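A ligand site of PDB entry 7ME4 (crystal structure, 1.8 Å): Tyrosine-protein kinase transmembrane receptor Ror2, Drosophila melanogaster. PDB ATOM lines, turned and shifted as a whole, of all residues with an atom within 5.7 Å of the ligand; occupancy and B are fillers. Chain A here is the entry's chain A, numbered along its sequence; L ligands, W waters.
Water W1 lies within hydrogen-bond range of an oxygen (O1) of the ligand and the backbone NH (N) of Ile 135.
Leu 65 touches the ligand (CD1 to C5, 3.8 Å). Ala 81 touches the ligand (CB to C14, 3.95 Å). Met 84 touches the ligand (CB to C11, 3.5 Å). CD1 of Leu 85 touches C7 of the ligand, 3.96 Å away. CG of Tyr 88 touches C8 of the ligand, at 3.6 Å. CG2 of Thr 113 touches C12 of the ligand, at 3.8 Å. CB of Cys 118 touches C16 of the ligand (3.8 Å). Asp 121 touches the ligand. Trp 122 touches the ligand. Ile 125 touches the ligand (CD1 to C16, 3.9 Å). Ile 135 touches the ligand. O of Phe 141 touches C3 of the ligand, at 3.7 Å. Arg 142 touches the ligand. CD of Pro 144 touches C10 of the ligand, at 3.9 Å. Of the 23 residues printed, 17 come within 4 Å of the ligand. Along chain A the residues within 4 Å of the ligand span positions 65 to 144.
The side-chain sulfur (SD) of Met 84 sits close to the side-chain hydroxyl (OG1) of Thr 113, at 3.7 Å. The backbone NH (N) of Arg 142 lies within hydrogen-bond range of the side-chain hydroxyl (OH) of Tyr 88. The side-chain sulfur (SG) of Cys 77 forms a disulfide with the side-chain sulfur (SG) of Cys 118 (2.2 Å). O of Thr 113 lies within hydrogen-bond range of N of Cys 118 (2.7 Å).
NZ of Lys 129 lies within salt-bridge range of O2 of the ligand, at 2.8 Å. O2 of the ligand sits at hydrogen-bond distance from N of Leu 143 (2.9 Å). The guanidinium group of Arg 138 is in salt-bridge range of an oxygen (O1) of the ligand (2.6 Å).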
ATOM      1  N   LEU A  65      -7.572  -6.216  -0.136  1.00  0.00           N
ATOM      2  CA  LEU A  65      -8.669  -5.921   0.803  1.00  0.00           C
ATOM      3  C   LEU A  65      -8.700  -6.908   1.960  1.00  0.00           C
ATOM      4  O   LEU A  65      -9.148  -6.560   3.069  1.00  0.00           O
ATOM      5  CB  LEU A  65     -10.011  -5.954   0.083  1.00  0.00           C
ATOM      6  CG  LEU A  65     -10.378  -4.699  -0.714  1.00  0.00           C
ATOM      7  CD1 LEU A  65     -11.667  -4.927  -1.460  1.00  0.00           C
ATOM      8  CD2 LEU A  65     -10.474  -3.482   0.255  1.00  0.00           C
ATOM      9  N   LEU A  69      -9.063  -4.640   4.896  1.00  0.00           N
ATOM     10  CA  LEU A  69     -10.430  -4.612   5.392  1.00  0.00           C
ATOM     11  C   LEU A  69     -10.792  -5.862   6.194  1.00  0.00           C
ATOM     12  O   LEU A  69     -11.183  -5.774   7.368  1.00  0.00           O
ATOM     13  CB  LEU A  69     -11.390  -4.417   4.212  1.00  0.00           C
ATOM     14  CG  LEU A  69     -12.862  -4.674   4.507  1.00  0.00           C
ATOM     15  CD1 LEU A  69     -13.362  -3.573   5.498  1.00  0.00           C
ATOM     16  CD2 LEU A  69     -13.648  -4.732   3.202  1.00  0.00           C
ATOM     17  N   LEU A  73     -11.867  -6.949  10.646  1.00  0.00           N
ATOM     18  CA  LEU A  73     -13.211  -7.314  11.057  1.00  0.00           C
ATOM     19  C   LEU A  73     -13.157  -8.509  12.000  1.00  0.00           C
ATOM     20  O   LEU A  73     -12.203  -9.286  11.984  1.00  0.00           O
ATOM     21  CB  LEU A  73     -14.045  -7.667   9.820  1.00  0.00           C
ATOM     22  CG  LEU A  73     -14.189  -6.558   8.770  1.00  0.00           C
ATOM     23  CD1 LEU A  73     -14.985  -7.078   7.522  1.00  0.00           C
ATOM     24  CD2 LEU A  73     -14.838  -5.283   9.378  1.00  0.00           C
ATOM     25  N   CYS A  77     -19.485 -10.433  11.736  1.00  0.00           N
ATOM     26  CA  CYS A  77     -19.210  -9.533  10.617  1.00  0.00           C
ATOM     27  C   CYS A  77     -18.112 -10.101   9.742  1.00  0.00           C
ATOM     28  O   CYS A  77     -18.248 -10.128   8.513  1.00  0.00           O
ATOM     29  CB  CYS A  77     -18.785  -8.128  11.110  1.00  0.00           C
ATOM     30  SG  CYS A  77     -18.409  -7.047   9.690  1.00  0.00           S
ATOM     31  N   ALA A  80     -19.343 -13.039   7.578  1.00  0.00           N
ATOM     32  CA  ALA A  80     -20.184 -12.620   6.460  1.00  0.00           C
ATOM     33  C   ALA A  80     -19.350 -11.922   5.399  1.00  0.00           C
ATOM     34  O   ALA A  80     -19.528 -12.179   4.195  1.00  0.00           O
ATOM     35  CB  ALA A  80     -21.302 -11.706   6.952  1.00  0.00           C
ATOM     36  N   ALA A  81     -18.438 -11.045   5.834  1.00  0.00           N
ATOM     37  CA  ALA A  81     -17.693 -10.213   4.909  1.00  0.00           C
ATOM     38  C   ALA A  81     -16.784 -11.047   4.030  1.00  0.00           C
ATOM     39  O   ALA A  81     -16.638 -10.752   2.848  1.00  0.00           O
ATOM     40  CB  ALA A  81     -16.871  -9.166   5.686  1.00  0.00           C
ATOM     41  N   MET A  84     -19.073 -12.664   1.429  1.00  0.00           N
ATOM     42  CA  MET A  84     -19.632 -11.649   0.551  1.00  0.00           C
ATOM     43  C   MET A  84     -18.555 -11.102  -0.357  1.00  0.00           C
ATOM     44  O   MET A  84     -18.803 -10.901  -1.538  1.00  0.00           O
ATOM     45  CB  MET A  84     -20.277 -10.503   1.364  1.00  0.00           C
ATOM     46  CG  MET A  84     -21.577 -10.977   1.996  1.00  0.00           C
ATOM     47  SD  MET A  84     -23.045 -10.816   0.942  1.00  0.00           S
ATOM     48  CE  MET A  84     -22.981  -9.029   0.669  1.00  0.00           C
ATOM     49  N   LEU A  85     -17.358 -10.817   0.201  1.00  0.00           N
ATOM     50  CA  LEU A  85     -16.292 -10.260  -0.622  1.00  0.00           C
ATOM     51  C   LEU A  85     -15.920 -11.227  -1.749  1.00  0.00           C
ATOM     52  O   LEU A  85     -15.707 -10.816  -2.902  1.00  0.00           O
ATOM     53  CB  LEU A  85     -15.053  -9.934   0.209  1.00  0.00           C
ATOM     54  CG  LEU A  85     -13.824  -9.425  -0.563  1.00  0.00           C
ATOM     55  CD1 LEU A  85     -14.157  -8.217  -1.499  1.00  0.00           C
ATOM     56  CD2 LEU A  85     -12.729  -9.047   0.443  1.00  0.00           C
ATOM     57  N   TYR A  88     -18.735 -11.338  -4.291  1.00  0.00           N
ATOM     58  CA  TYR A  88     -18.713 -10.117  -5.082  1.00  0.00           C
ATOM     59  C   TYR A  88     -17.587 -10.135  -6.124  1.00  0.00           C
ATOM     60  O   TYR A  88     -17.792  -9.740  -7.281  1.00  0.00           O
ATOM     61  CB  TYR A  88     -18.530  -8.922  -4.148  1.00  0.00           C
ATOM     62  CG  TYR A  88     -18.397  -7.570  -4.814  1.00  0.00           C
ATOM     63  CD1 TYR A  88     -19.517  -6.792  -5.098  1.00  0.00           C
ATOM     64  CD2 TYR A  88     -17.144  -7.063  -5.120  1.00  0.00           C
ATOM     65  CE1 TYR A  88     -19.391  -5.524  -5.674  1.00  0.00           C
ATOM     66  CE2 TYR A  88     -17.005  -5.793  -5.693  1.00  0.00           C
ATOM     67  CZ  TYR A  88     -18.129  -5.044  -5.971  1.00  0.00           C
ATOM     68  OH  TYR A  88     -17.987  -3.814  -6.532  1.00  0.00           O
ATOM     69  N   LEU A 105     -24.675 -10.588  -6.366  1.00  0.00           N
ATOM     70  CA  LEU A 105     -24.980 -10.924  -4.984  1.00  0.00           C
ATOM     71  C   LEU A 105     -26.481 -10.979  -4.785  1.00  0.00           C
ATOM     72  O   LEU A 105     -27.228 -10.292  -5.492  1.00  0.00           O
ATOM     73  CB  LEU A 105     -24.403  -9.818  -4.075  1.00  0.00           C
ATOM     74  CG  LEU A 105     -22.887  -9.751  -4.033  1.00  0.00           C
ATOM     75  CD1 LEU A 105     -22.474  -8.450  -3.266  1.00  0.00           C
ATOM     76  CD2 LEU A 105     -22.314 -10.993  -3.366  1.00  0.00           C
ATOM     77  N   THR A 113     -25.860  -8.699   5.703  1.00  0.00           N
ATOM     78  CA  THR A 113     -24.539  -8.147   5.977  1.00  0.00           C
ATOM     79  C   THR A 113     -24.643  -6.678   6.348  1.00  0.00           C
ATOM     80  O   THR A 113     -24.085  -6.258   7.357  1.00  0.00           O
ATOM     81  CB  THR A 113     -23.614  -8.364   4.760  1.00  0.00           C
ATOM     82  OG1 THR A 113     -23.572  -9.771   4.476  1.00  0.00           O
ATOM     83  CG2 THR A 113     -22.189  -7.854   5.081  1.00  0.00           C
ATOM     84  N   CYS A 118     -22.730  -6.645   9.707  1.00  0.00           N
ATOM     85  CA  CYS A 118     -21.620  -5.714   9.513  1.00  0.00           C
ATOM     86  C   CYS A 118     -22.082  -4.278   9.622  1.00  0.00           C
ATOM     87  O   CYS A 118     -21.377  -3.397   9.162  1.00  0.00           O
ATOM     88  CB  CYS A 118     -20.927  -5.884   8.154  1.00  0.00           C
ATOM     89  SG  CYS A 118     -19.882  -7.444   8.150  1.00  0.00           S
ATOM     90  N   ASP A 121     -19.530  -1.609  11.168  1.00  0.00           N
ATOM     91  CA  ASP A 121     -18.383  -1.424  10.292  1.00  0.00           C
ATOM     92  C   ASP A 121     -18.769  -0.775   8.969  1.00  0.00           C
ATOM     93  O   ASP A 121     -18.022   0.045   8.444  1.00  0.00           O
ATOM     94  CB  ASP A 121     -17.714  -2.774  10.072  1.00  0.00           C
ATOM     95  CG  ASP A 121     -16.774  -3.131  11.238  1.00  0.00           C
ATOM     96  OD1 ASP A 121     -15.771  -2.433  11.406  1.00  0.00           O
ATOM     97  OD2 ASP A 121     -17.080  -4.050  12.016  1.00  0.00           O
ATOM     98  N   TRP A 122     -19.914  -1.166   8.402  1.00  0.00           N
ATOM     99  CA  TRP A 122     -20.414  -0.592   7.150  1.00  0.00           C
ATOM    100  C   TRP A 122     -20.702   0.888   7.271  1.00  0.00           C
ATOM    101  O   TRP A 122     -20.216   1.705   6.456  1.00  0.00           O
ATOM    102  CB  TRP A 122     -21.679  -1.378   6.712  1.00  0.00           C
ATOM    103  CG  TRP A 122     -22.168  -1.144   5.334  1.00  0.00           C
ATOM    104  CD1 TRP A 122     -22.625   0.025   4.790  1.00  0.00           C
ATOM    105  CD2 TRP A 122     -22.413  -2.171   4.351  1.00  0.00           C
ATOM    106  NE1 TRP A 122     -23.080  -0.201   3.500  1.00  0.00           N
ATOM    107  CE2 TRP A 122     -22.982  -1.542   3.225  1.00  0.00           C
ATOM    108  CE3 TRP A 122     -22.202  -3.537   4.320  1.00  0.00           C
ATOM    109  CZ2 TRP A 122     -23.320  -2.244   2.058  1.00  0.00           C
ATOM    110  CZ3 TRP A 122     -22.556  -4.259   3.139  1.00  0.00           C
ATOM    111  CH2 TRP A 122     -23.099  -3.601   2.046  1.00  0.00           C
ATOM    112  N   ILE A 125     -17.398   2.871   7.494  1.00  0.00           N
ATOM    113  CA  ILE A 125     -16.807   3.045   6.170  1.00  0.00           C
ATOM    114  C   ILE A 125     -17.554   4.127   5.388  1.00  0.00           C
ATOM    115  O   ILE A 125     -16.944   5.005   4.787  1.00  0.00           O
ATOM    116  CB  ILE A 125     -16.795   1.714   5.403  1.00  0.00           C
ATOM    117  CG1 ILE A 125     -15.842   0.713   6.082  1.00  0.00           C
ATOM    118  CG2 ILE A 125     -16.471   1.972   3.943  1.00  0.00           C
ATOM    119  CD1 ILE A 125     -16.027  -0.798   5.512  1.00  0.00           C
ATOM    120  N   LYS A 129     -16.138   7.605   3.729  1.00  0.00           N
ATOM    121  CA  LYS A 129     -16.298   7.939   2.311  1.00  0.00           C
ATOM    122  C   LYS A 129     -16.874   9.328   2.111  1.00  0.00           C
ATOM    123  O   LYS A 129     -16.524  10.020   1.149  1.00  0.00           O
ATOM    124  CB  LYS A 129     -17.235   6.934   1.648  1.00  0.00           C
ATOM    125  CG  LYS A 129     -16.617   5.605   1.306  1.00  0.00           C
ATOM    126  CD  LYS A 129     -17.705   4.679   0.764  1.00  0.00           C
ATOM    127  CE  LYS A 129     -17.835   4.807  -0.746  1.00  0.00           C
ATOM    128  NZ  LYS A 129     -18.600   3.652  -1.300  1.00  0.00           N
ATOM    129  N   PHE A 134     -11.083   6.858   1.863  1.00  0.00           N
ATOM    130  CA  PHE A 134     -11.455   5.572   1.282  1.00  0.00           C
ATOM    131  C   PHE A 134     -10.496   4.466   1.705  1.00  0.00           C
ATOM    132  O   PHE A 134      -9.333   4.717   2.053  1.00  0.00           O
ATOM    133  CB  PHE A 134     -11.479   5.650  -0.255  1.00  0.00           C
ATOM    134  CG  PHE A 134     -12.309   6.774  -0.790  1.00  0.00           C
ATOM    135  CD1 PHE A 134     -13.693   6.719  -0.704  1.00  0.00           C
ATOM    136  CD2 PHE A 134     -11.705   7.883  -1.363  1.00  0.00           C
ATOM    137  CE1 PHE A 134     -14.460   7.769  -1.181  1.00  0.00           C
ATOM    138  CE2 PHE A 134     -12.471   8.916  -1.838  1.00  0.00           C
ATOM    139  CZ  PHE A 134     -13.850   8.863  -1.740  1.00  0.00           C
ATOM    140  N   ILE A 135     -11.010   3.240   1.688  1.00  0.00           N
ATOM    141  CA  ILE A 135     -10.158   2.085   1.883  1.00  0.00           C
ATOM    142  C   ILE A 135      -9.149   2.109   0.745  1.00  0.00           C
ATOM    143  O   ILE A 135      -9.533   2.167  -0.431  1.00  0.00           O
ATOM    144  CB  ILE A 135     -10.996   0.793   1.892  1.00  0.00           C
ATOM    145  CG1 ILE A 135     -11.791   0.702   3.202  1.00  0.00           C
ATOM    146  CG2 ILE A 135     -10.112  -0.428   1.785  1.00  0.00           C
ATOM    147  CD1 ILE A 135     -13.144   0.104   3.013  1.00  0.00           C
ATOM    148  N   ARG A 138      -9.326  -0.543  -2.190  1.00  0.00           N
ATOM    149  CA  ARG A 138     -10.603  -0.972  -2.760  1.00  0.00           C
ATOM    150  C   ARG A 138     -10.582  -1.076  -4.292  1.00  0.00           C
ATOM    151  O   ARG A 138     -11.419  -1.789  -4.844  1.00  0.00           O
ATOM    152  CB  ARG A 138     -11.744  -0.051  -2.337  1.00  0.00           C
ATOM    153  CG  ARG A 138     -11.648   1.328  -2.980  1.00  0.00           C
ATOM    154  CD  ARG A 138     -12.602   2.321  -2.305  1.00  0.00           C
ATOM    155  NE  ARG A 138     -12.574   3.589  -3.045  1.00  0.00           N
ATOM    156  CZ  ARG A 138     -13.617   4.375  -3.279  1.00  0.00           C
ATOM    157  NH1 ARG A 138     -14.819   4.061  -2.809  1.00  0.00           N
ATOM    158  NH2 ARG A 138     -13.437   5.501  -3.965  1.00  0.00           N
ATOM    159  N   PHE A 141     -13.721  -1.828  -6.466  1.00  0.00           N
ATOM    160  CA  PHE A 141     -14.764  -2.472  -5.668  1.00  0.00           C
ATOM    161  C   PHE A 141     -15.535  -1.419  -4.889  1.00  0.00           C
ATOM    162  O   PHE A 141     -14.943  -0.459  -4.400  1.00  0.00           O
ATOM    163  CB  PHE A 141     -14.162  -3.476  -4.686  1.00  0.00           C
ATOM    164  CG  PHE A 141     -13.711  -4.779  -5.300  1.00  0.00           C
ATOM    165  CD1 PHE A 141     -13.512  -4.890  -6.663  1.00  0.00           C
ATOM    166  CD2 PHE A 141     -13.455  -5.890  -4.481  1.00  0.00           C
ATOM    167  CE1 PHE A 141     -13.087  -6.083  -7.218  1.00  0.00           C
ATOM    168  CE2 PHE A 141     -13.047  -7.064  -5.003  1.00  0.00           C
ATOM    169  CZ  PHE A 141     -12.856  -7.180  -6.393  1.00  0.00           C
ATOM    170  N   ARG A 142     -16.834  -1.615  -4.735  1.00  0.00           N
ATOM    171  CA  ARG A 142     -17.660  -0.686  -3.965  1.00  0.00           C
ATOM    172  C   ARG A 142     -18.693  -1.429  -3.118  1.00  0.00           C
ATOM    173  O   ARG A 142     -19.170  -2.498  -3.493  1.00  0.00           O
ATOM    174  CB  ARG A 142     -18.388   0.311  -4.898  1.00  0.00           C
ATOM    175  CG  ARG A 142     -17.504   1.197  -5.786  1.00  0.00           C
ATOM    176  CD  ARG A 142     -16.813   2.278  -4.994  1.00  0.00           C
ATOM    177  NE  ARG A 142     -16.043   3.198  -5.841  1.00  0.00           N
ATOM    178  CZ  ARG A 142     -14.800   2.996  -6.256  1.00  0.00           C
ATOM    179  NH1 ARG A 142     -14.121   1.906  -5.894  1.00  0.00           N
ATOM    180  NH2 ARG A 142     -14.212   3.900  -7.019  1.00  0.00           N
ATOM    181  N   LEU A 143     -19.049  -0.854  -1.960  1.00  0.00           N
ATOM    182  CA  LEU A 143     -20.125  -1.451  -1.173  1.00  0.00           C
ATOM    183  C   LEU A 143     -21.384  -1.536  -2.018  1.00  0.00           C
ATOM    184  O   LEU A 143     -21.779  -0.545  -2.645  1.00  0.00           O
ATOM    185  CB  LEU A 143     -20.411  -0.607   0.080  1.00  0.00           C
ATOM    186  CG  LEU A 143     -19.318  -0.639   1.139  1.00  0.00           C
ATOM    187  CD1 LEU A 143     -19.649   0.463   2.233  1.00  0.00           C
ATOM    188  CD2 LEU A 143     -19.242  -2.035   1.737  1.00  0.00           C
ATOM    189  N   PRO A 144     -22.040  -2.686  -2.067  1.00  0.00           N
ATOM    190  CA  PRO A 144     -23.234  -2.817  -2.919  1.00  0.00           C
ATOM    191  C   PRO A 144     -24.437  -2.131  -2.290  1.00  0.00           C
ATOM    192  O   PRO A 144     -24.529  -1.948  -1.070  1.00  0.00           O
ATOM    193  CB  PRO A 144     -23.469  -4.328  -2.985  1.00  0.00           C
ATOM    194  CG  PRO A 144     -22.812  -4.881  -1.840  1.00  0.00           C
ATOM    195  CD  PRO A 144     -21.724  -3.932  -1.353  1.00  0.00           C
HETATM  196  C1  LIG L   1     -16.083   1.393  -0.651  1.00  0.00           C
HETATM  197  O1  LIG L   1     -15.536   2.499  -0.793  1.00  0.00           O
HETATM  198  O2  LIG L   1     -17.263   1.241  -1.084  1.00  0.00           O
HETATM  199  C2  LIG L   1     -15.316   0.276   0.054  1.00  0.00           C
HETATM  200  C3  LIG L   1     -15.371  -1.006  -0.774  1.00  0.00           C
HETATM  201  C4  LIG L   1     -14.899  -2.217   0.049  1.00  0.00           C
HETATM  202  C5  LIG L   1     -15.134  -3.513  -0.740  1.00  0.00           C
HETATM  203  C6  LIG L   1     -16.614  -3.823  -0.953  1.00  0.00           C
HETATM  204  C7  LIG L   1     -16.718  -5.203  -1.577  1.00  0.00           C
HETATM  205  C8  LIG L   1     -18.163  -5.730  -1.679  1.00  0.00           C
HETATM  206  C9  LIG L   1     -18.479  -6.690  -0.530  1.00  0.00           C
HETATM  207  C10 LIG L   1     -19.182  -6.220   0.501  1.00  0.00           C
HETATM  208  C11 LIG L   1     -19.502  -7.104   1.693  1.00  0.00           C
HETATM  209  C12 LIG L   1     -19.390  -6.286   2.969  1.00  0.00           C
HETATM  210  C13 LIG L   1     -18.028  -5.617   3.107  1.00  0.00           C
HETATM  211  C14 LIG L   1     -17.690  -5.458   4.588  1.00  0.00           C
HETATM  212  C15 LIG L   1     -18.250  -4.129   5.077  1.00  0.00           C
HETATM  213  C16 LIG L   1     -17.972  -4.064   6.554  1.00  0.00           C
HETATM  214  O   HOH W   1     -13.835   3.332   1.179  1.00  0.00           O
